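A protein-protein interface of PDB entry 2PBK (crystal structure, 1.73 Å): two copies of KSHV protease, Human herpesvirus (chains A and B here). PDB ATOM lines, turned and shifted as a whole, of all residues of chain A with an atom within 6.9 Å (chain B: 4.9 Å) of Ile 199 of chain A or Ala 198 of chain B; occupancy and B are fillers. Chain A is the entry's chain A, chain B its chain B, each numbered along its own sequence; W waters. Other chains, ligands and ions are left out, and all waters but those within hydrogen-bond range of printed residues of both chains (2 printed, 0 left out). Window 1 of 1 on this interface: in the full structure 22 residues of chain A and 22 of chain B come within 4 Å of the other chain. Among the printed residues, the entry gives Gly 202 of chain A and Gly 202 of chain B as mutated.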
ATOM      1  N   GLU A 192      18.088 -13.891 -14.813  1.00  0.00           N
ATOM      2  CA  GLU A 192      19.323 -13.499 -15.567  1.00  0.00           C
ATOM      3  C   GLU A 192      19.213 -13.704 -17.086  1.00  0.00           C
ATOM      4  O   GLU A 192      19.697 -12.876 -17.870  1.00  0.00           O
ATOM      5  CB  GLU A 192      20.570 -14.226 -15.078  1.00  0.00           C
ATOM      6  CG  GLU A 192      20.935 -13.894 -13.689  1.00  0.00           C
ATOM      7  CD  GLU A 192      20.352 -14.827 -12.666  1.00  0.00           C
ATOM      8  OE1 GLU A 192      19.233 -15.410 -12.838  1.00  0.00           O
ATOM      9  OE2 GLU A 192      21.044 -14.967 -11.637  1.00  0.00           O
ATOM     10  N   LEU A 194      16.456 -13.531 -18.822  1.00  0.00           N
ATOM     11  CA  LEU A 194      15.562 -12.481 -19.318  1.00  0.00           C
ATOM     12  C   LEU A 194      16.303 -11.122 -19.328  1.00  0.00           C
ATOM     13  O   LEU A 194      16.120 -10.302 -20.237  1.00  0.00           O
ATOM     14  CB  LEU A 194      14.298 -12.405 -18.465  1.00  0.00           C
ATOM     15  CG  LEU A 194      13.412 -13.652 -18.531  1.00  0.00           C
ATOM     16  CD1 LEU A 194      12.254 -13.513 -17.542  1.00  0.00           C
ATOM     17  CD2 LEU A 194      12.911 -13.897 -19.901  1.00  0.00           C
ATOM     18  N   MET A 195      17.122 -10.899 -18.321  1.00  0.00           N
ATOM     19  CA  MET A 195      17.817  -9.613 -18.210  1.00  0.00           C
ATOM     20  C   MET A 195      18.847  -9.482 -19.320  1.00  0.00           C
ATOM     21  O   MET A 195      19.038  -8.399 -19.842  1.00  0.00           O
ATOM     22  CB  MET A 195      18.499  -9.420 -16.869  1.00  0.00           C
ATOM     23  CG  MET A 195      19.099  -8.003 -16.718  1.00  0.00           C
ATOM     24  SD  MET A 195      19.543  -7.621 -15.025  1.00  0.00           S
ATOM     25  CE  MET A 195      20.628  -8.990 -14.614  1.00  0.00           C
ATOM     26  N   ALA A 196      19.507 -10.589 -19.671  1.00  0.00           N
ATOM     27  CA  ALA A 196      20.452 -10.586 -20.810  1.00  0.00           C
ATOM     28  C   ALA A 196      19.738 -10.196 -22.106  1.00  0.00           C
ATOM     29  O   ALA A 196      20.253  -9.426 -22.912  1.00  0.00           O
ATOM     30  CB  ALA A 196      21.087 -11.970 -20.933  1.00  0.00           C
ATOM     31  N   LYS A 197      18.542 -10.715 -22.330  1.00  0.00           N
ATOM     32  CA  LYS A 197      17.755 -10.317 -23.482  1.00  0.00           C
ATOM     33  C   LYS A 197      17.360  -8.843 -23.430  1.00  0.00           C
ATOM     34  O   LYS A 197      17.395  -8.158 -24.468  1.00  0.00           O
ATOM     35  CB  LYS A 197      16.475 -11.146 -23.587  1.00  0.00           C
ATOM     36  CG  LYS A 197      16.714 -12.499 -24.127  1.00  0.00           C
ATOM     37  CD  LYS A 197      16.951 -12.432 -25.644  1.00  0.00           C
ATOM     38  CE  LYS A 197      17.003 -13.802 -26.273  1.00  0.00           C
ATOM     39  NZ  LYS A 197      17.661 -13.688 -27.599  1.00  0.00           N
ATOM     40  N   ALA A 198      17.017  -8.352 -22.240  1.00  0.00           N
ATOM     41  CA  ALA A 198      16.633  -6.913 -22.062  1.00  0.00           C
ATOM     42  C   ALA A 198      17.811  -5.972 -22.369  1.00  0.00           C
ATOM     43  O   ALA A 198      17.644  -4.883 -22.956  1.00  0.00           O
ATOM     44  CB  ALA A 198      16.139  -6.662 -20.665  1.00  0.00           C
ATOM     45  N   ILE A 199      18.987  -6.382 -21.946  1.00  0.00           N
ATOM     46  CA  ILE A 199      20.228  -5.675 -22.223  1.00  0.00           C
ATOM     47  C   ILE A 199      20.495  -5.656 -23.731  1.00  0.00           C
ATOM     48  O   ILE A 199      20.865  -4.616 -24.298  1.00  0.00           O
ATOM     49  CB  ILE A 199      21.383  -6.291 -21.437  1.00  0.00           C
ATOM     50  CG1 ILE A 199      21.231  -5.978 -19.952  1.00  0.00           C
ATOM     51  CG2 ILE A 199      22.760  -5.833 -21.947  1.00  0.00           C
ATOM     52  CD1 ILE A 199      22.161  -6.745 -19.057  1.00  0.00           C
ATOM     53  N   ASP A 200      20.364  -6.820 -24.381  1.00  0.00           N
ATOM     54  CA  ASP A 200      20.593  -6.917 -25.818  1.00  0.00           C
ATOM     55  C   ASP A 200      19.640  -5.993 -26.582  1.00  0.00           C
ATOM     56  O   ASP A 200      20.039  -5.393 -27.590  1.00  0.00           O
ATOM     57  CB  ASP A 200      20.379  -8.381 -26.322  1.00  0.00           C
ATOM     58  CG  ASP A 200      21.516  -9.320 -25.977  1.00  0.00           C
ATOM     59  OD1 ASP A 200      22.639  -8.855 -25.649  1.00  0.00           O
ATOM     60  OD2 ASP A 200      21.295 -10.585 -26.098  1.00  0.00           O
ATOM     61  N   ALA A 201      18.403  -5.894 -26.081  1.00  0.00           N
ATOM     62  CA  ALA A 201      17.310  -5.094 -26.681  1.00  0.00           C
ATOM     63  C   ALA A 201      17.738  -3.646 -26.880  1.00  0.00           C
ATOM     64  O   ALA A 201      17.442  -3.020 -27.915  1.00  0.00           O
ATOM     65  CB  ALA A 201      16.046  -5.179 -25.865  1.00  0.00           C
ATOM     66  N   GLY A 202      18.509  -3.146 -25.927  1.00  0.00           N
ATOM     67  CA  GLY A 202      18.949  -1.770 -26.031  1.00  0.00           C
ATOM     68  C   GLY A 202      19.865  -1.510 -27.227  1.00  0.00           C
ATOM     69  O   GLY A 202      20.033  -0.364 -27.628  1.00  0.00           O
ATOM     70  N   PHE A 203      20.484  -2.553 -27.796  1.00  0.00           N
ATOM     71  CA  PHE A 203      21.386  -2.381 -28.948  1.00  0.00           C
ATOM     72  C   PHE A 203      20.770  -2.659 -30.298  1.00  0.00           C
ATOM     73  O   PHE A 203      21.478  -2.558 -31.306  1.00  0.00           O
ATOM     74  CB  PHE A 203      22.615  -3.247 -28.804  1.00  0.00           C
ATOM     75  CG  PHE A 203      23.496  -2.801 -27.727  1.00  0.00           C
ATOM     76  CD1 PHE A 203      24.565  -1.963 -27.980  1.00  0.00           C
ATOM     77  CD2 PHE A 203      23.234  -3.224 -26.424  1.00  0.00           C
ATOM     78  CE1 PHE A 203      25.379  -1.540 -26.969  1.00  0.00           C
ATOM     79  CE2 PHE A 203      24.054  -2.814 -25.398  1.00  0.00           C
ATOM     80  CZ  PHE A 203      25.106  -1.976 -25.656  1.00  0.00           C
ATOM     81  N   ILE A 204      19.481  -2.962 -30.310  1.00  0.00           N
ATOM     82  CA  ILE A 204      18.762  -3.192 -31.541  1.00  0.00           C
ATOM     83  C   ILE A 204      18.684  -1.872 -32.305  1.00  0.00           C
ATOM     84  O   ILE A 204      18.168  -0.852 -31.838  1.00  0.00           O
ATOM     85  CB  ILE A 204      17.376  -3.811 -31.322  1.00  0.00           C
ATOM     86  CG1 ILE A 204      17.465  -5.207 -30.660  1.00  0.00           C
ATOM     87  CG2 ILE A 204      16.647  -3.870 -32.663  1.00  0.00           C
ATOM     88  CD1 ILE A 204      16.130  -5.769 -30.112  1.00  0.00           C
ATOM     89  N   LEU B  81      25.408 -13.343 -17.244  1.00  0.00           N
ATOM     90  CA  LEU B  81      24.794 -12.530 -18.288  1.00  0.00           C
ATOM     91  C   LEU B  81      25.552 -12.661 -19.621  1.00  0.00           C
ATOM     92  O   LEU B  81      24.944 -12.744 -20.674  1.00  0.00           O
ATOM     93  CB  LEU B  81      24.743 -11.078 -17.852  1.00  0.00           C
ATOM     94  CG  LEU B  81      23.806 -10.752 -16.694  1.00  0.00           C
ATOM     95  CD1 LEU B  81      24.011  -9.301 -16.226  1.00  0.00           C
ATOM     96  CD2 LEU B  81      22.322 -11.018 -17.060  1.00  0.00           C
ATOM     97  N   THR B 106      28.562  -3.798 -22.711  1.00  0.00           N
ATOM     98  CA  THR B 106      27.204  -3.903 -23.193  1.00  0.00           C
ATOM     99  C   THR B 106      26.169  -3.417 -22.174  1.00  0.00           C
ATOM    100  O   THR B 106      25.238  -2.707 -22.510  1.00  0.00           O
ATOM    101  CB  THR B 106      26.909  -5.389 -23.534  1.00  0.00           C
ATOM    102  OG1 THR B 106      27.910  -5.900 -24.424  1.00  0.00           O
ATOM    103  CG2 THR B 106      25.530  -5.557 -24.157  1.00  0.00           C
ATOM    104  N   TRP B 107      26.349  -3.835 -20.929  1.00  0.00           N
ATOM    105  CA  TRP B 107      25.393  -3.547 -19.826  1.00  0.00           C
ATOM    106  C   TRP B 107      25.619  -2.159 -19.189  1.00  0.00           C
ATOM    107  O   TRP B 107      24.699  -1.423 -18.918  1.00  0.00           O
ATOM    108  CB  TRP B 107      25.557  -4.650 -18.825  1.00  0.00           C
ATOM    109  CG  TRP B 107      24.702  -4.609 -17.582  1.00  0.00           C
ATOM    110  CD1 TRP B 107      23.540  -3.914 -17.378  1.00  0.00           C
ATOM    111  CD2 TRP B 107      24.982  -5.296 -16.375  1.00  0.00           C
ATOM    112  NE1 TRP B 107      23.066  -4.138 -16.112  1.00  0.00           N
ATOM    113  CE2 TRP B 107      23.933  -4.987 -15.462  1.00  0.00           C
ATOM    114  CE3 TRP B 107      25.993  -6.173 -15.974  1.00  0.00           C
ATOM    115  CZ2 TRP B 107      23.918  -5.479 -14.186  1.00  0.00           C
ATOM    116  CZ3 TRP B 107      25.956  -6.682 -14.691  1.00  0.00           C
ATOM    117  CH2 TRP B 107      24.934  -6.327 -13.812  1.00  0.00           C
ATOM    118  N   LEU B 194      17.866  -4.267 -10.902  1.00  0.00           N
ATOM    119  CA  LEU B 194      18.795  -4.153 -12.033  1.00  0.00           C
ATOM    120  C   LEU B 194      18.092  -4.421 -13.374  1.00  0.00           C
ATOM    121  O   LEU B 194      18.391  -3.745 -14.361  1.00  0.00           O
ATOM    122  CB  LEU B 194      19.960  -5.139 -11.865  1.00  0.00           C
ATOM    123  CG  LEU B 194      20.915  -4.795 -10.698  1.00  0.00           C
ATOM    124  CD1 LEU B 194      21.941  -5.898 -10.485  1.00  0.00           C
ATOM    125  CD2 LEU B 194      21.568  -3.485 -10.930  1.00  0.00           C
ATOM    126  N   MET B 195      17.170  -5.393 -13.395  1.00  0.00           N
ATOM    127  CA  MET B 195      16.451  -5.709 -14.666  1.00  0.00           C
ATOM    128  C   MET B 195      15.583  -4.512 -15.024  1.00  0.00           C
ATOM    129  O   MET B 195      15.554  -4.135 -16.192  1.00  0.00           O
ATOM    130  CB  MET B 195      15.613  -6.991 -14.639  1.00  0.00           C
ATOM    131  CG  MET B 195      15.303  -7.659 -16.185  1.00  0.00           C
ATOM    132  SD  MET B 195      14.460  -9.135 -15.659  1.00  0.00           S
ATOM    133  CE  MET B 195      13.080  -8.535 -14.711  1.00  0.00           C
ATOM    134  N   ALA B 196      14.877  -3.921 -14.051  1.00  0.00           N
ATOM    135  CA  ALA B 196      14.055  -2.707 -14.313  1.00  0.00           C
ATOM    136  C   ALA B 196      14.889  -1.576 -14.942  1.00  0.00           C
ATOM    137  O   ALA B 196      14.480  -0.917 -15.919  1.00  0.00           O
ATOM    138  CB  ALA B 196      13.327  -2.232 -13.023  1.00  0.00           C
ATOM    139  N   LYS B 197      16.082  -1.368 -14.410  1.00  0.00           N
ATOM    140  CA  LYS B 197      16.949  -0.349 -14.938  1.00  0.00           C
ATOM    141  C   LYS B 197      17.403  -0.659 -16.388  1.00  0.00           C
ATOM    142  O   LYS B 197      17.491   0.228 -17.219  1.00  0.00           O
ATOM    143  CB  LYS B 197      18.138  -0.136 -13.991  1.00  0.00           C
ATOM    144  CG  LYS B 197      17.719   0.494 -12.648  1.00  0.00           C
ATOM    145  CD  LYS B 197      18.912   1.027 -11.885  1.00  0.00           C
ATOM    146  CE  LYS B 197      18.511   1.644 -10.541  1.00  0.00           C
ATOM    147  NZ  LYS B 197      18.052   3.045 -10.713  1.00  0.00           N
ATOM    148  N   ALA B 198      17.709  -1.930 -16.655  1.00  0.00           N
ATOM    149  CA  ALA B 198      18.098  -2.370 -17.992  1.00  0.00           C
ATOM    150  C   ALA B 198      16.936  -2.168 -18.990  1.00  0.00           C
ATOM    151  O   ALA B 198      17.149  -1.741 -20.117  1.00  0.00           O
ATOM    152  CB  ALA B 198      18.522  -3.842 -17.960  1.00  0.00           C
ATOM    153  N   ILE B 199      15.717  -2.480 -18.561  1.00  0.00           N
ATOM    154  CA  ILE B 199      14.522  -2.245 -19.382  1.00  0.00           C
ATOM    155  C   ILE B 199      14.368  -0.752 -19.688  1.00  0.00           C
ATOM    156  O   ILE B 199      14.189  -0.336 -20.851  1.00  0.00           O
ATOM    157  CB  ILE B 199      13.266  -2.784 -18.681  1.00  0.00           C
ATOM    158  CG1 ILE B 199      13.282  -4.343 -18.654  1.00  0.00           C
ATOM    159  CG2 ILE B 199      12.008  -2.281 -19.377  1.00  0.00           C
ATOM    160  CD1 ILE B 199      12.325  -4.953 -17.768  1.00  0.00           C
ATOM    161  N   ASP B 200      14.456   0.059 -18.653  1.00  0.00           N
ATOM    162  CA  ASP B 200      14.349   1.515 -18.844  1.00  0.00           C
ATOM    163  C   ASP B 200      15.425   2.050 -19.791  1.00  0.00           C
ATOM    164  O   ASP B 200      15.151   2.911 -20.581  1.00  0.00           O
ATOM    165  CB  ASP B 200      14.482   2.263 -17.494  1.00  0.00           C
ATOM    166  CG  ASP B 200      13.247   2.166 -16.612  1.00  0.00           C
ATOM    167  OD1 ASP B 200      12.161   1.742 -17.062  1.00  0.00           O
ATOM    168  OD2 ASP B 200      13.380   2.549 -15.411  1.00  0.00           O
ATOM    169  N   ALA B 201      16.637   1.521 -19.703  1.00  0.00           N
ATOM    170  CA  ALA B 201      17.778   1.998 -20.495  1.00  0.00           C
ATOM    171  C   ALA B 201      17.495   1.822 -21.996  1.00  0.00           C
ATOM    172  O   ALA B 201      17.849   2.674 -22.801  1.00  0.00           O
ATOM    173  CB  ALA B 201      19.034   1.261 -20.100  1.00  0.00           C
ATOM    174  N   GLY B 202      16.774   0.765 -22.359  1.00  0.00           N
ATOM    175  CA  GLY B 202      16.392   0.553 -23.755  1.00  0.00           C
ATOM    176  C   GLY B 202      15.485   1.627 -24.351  1.00  0.00           C
ATOM    177  O   GLY B 202      15.420   1.818 -25.591  1.00  0.00           O
HETATM  178  O   HOH W   1      18.232  -2.289 -22.467  1.00  0.00           O
HETATM  179  O   HOH W   2      15.805  -0.006 -27.297  1.00  0.00           O
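SD of Met 195 of chain A sits at hydrogen-bond distance from N of Met 195 of chain B, 3.6 Å away.
Glu 192 of chain A touches Leu 81 of chain B. Leu 81 of chain B touches Met 195 of chain A (CD2 to CE, 3.6 Å). C of Leu 194 of chain B touches SD of Met 195 of chain A (3.9 Å). Ala 196 of chain A touches Leu 81 of chain B (N to CD2, 3.9 Å). CG2 of Thr 106 of chain B touches CG2 of Ile 199 of chain A (3.6 Å). Trp 107 of chain B touches Ile 199 of chain A (CD1 to CD1, 3.6 Å). Ile 199 of chain A touches Ala 198 of chain B (CG1 to CB, 3.98 Å). Thr 106 of chain B touches Phe 203 of chain A (O to CE2, 3.1 Å).
Of the printed residues of chain B, Ile 199 of chain A touches Thr 106 (3.6 Å), Trp 107 (3.6 Å) and Ala 198 (3.98 Å). Of the printed residues of chain A, Ala 198 of chain B touches Ile 199. Printed residues of chain A within 4 Å of Met 195 of chain B: Met 195. Of the printed residues of chain A, Leu 81 of chain B touches Glu 192 (3.3 Å), Met 195 (3.6 Å) and Ala 196 (3.9 Å). Ala 196 of chain B touches none of the printed residues of chain A. The nearest printed residue of chain B that does not touch Ile 199 of chain A is Leu 81 of chain B (4.2 Å).
Hydrophobic or aromatic side chains of chain A that line the printed part of chain B: Met 195, Ala 196, Ile 199 and Phe 203. Of the 12 printed residues of chain B, 6 touch a printed residue of chain A. Hydrophobic or aromatic side chains of chain B within 4 Å of the printed part of chain A: Leu 81, Trp 107, Met 195 and Ala 198. Among the printed residues, no Asp or Glu carboxylate lies within 4 Å of a Lys or Arg side-chain nitrogen of the other chain.
Met 195 of chain A touches Leu 194 of chain B, but with the chains exchanged Leu 194 of chain A does not touch Met 195 of chain B (4.3 Å). Met 195 of chain A touches its own counterpart, Met 195 of chain B. Ile 199 of chain A touches Ala 198 of chain B, but with the chains exchanged Ala 198 of chain A does not touch Ile 199 of chain B (4.2 Å). Of the 9 pairs that touch across the chains among the printed residues, 1 has its exchanged pair printed and touching as well.
Water W2 lies within hydrogen-bond range of the backbone carbonyl oxygen (O) of Gly 202 of chain B (2.5 Å) and the backbone carbonyl oxygen (O) of Ala 201 of chain A (3.5 Å). Water W1 lies within hydrogen-bond range of the backbone carbonyl oxygen of Ala 198 of chain B, the backbone carbonyl oxygen of Ala 198 of chain A and the backbone NH of Gly 202 of chain B.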
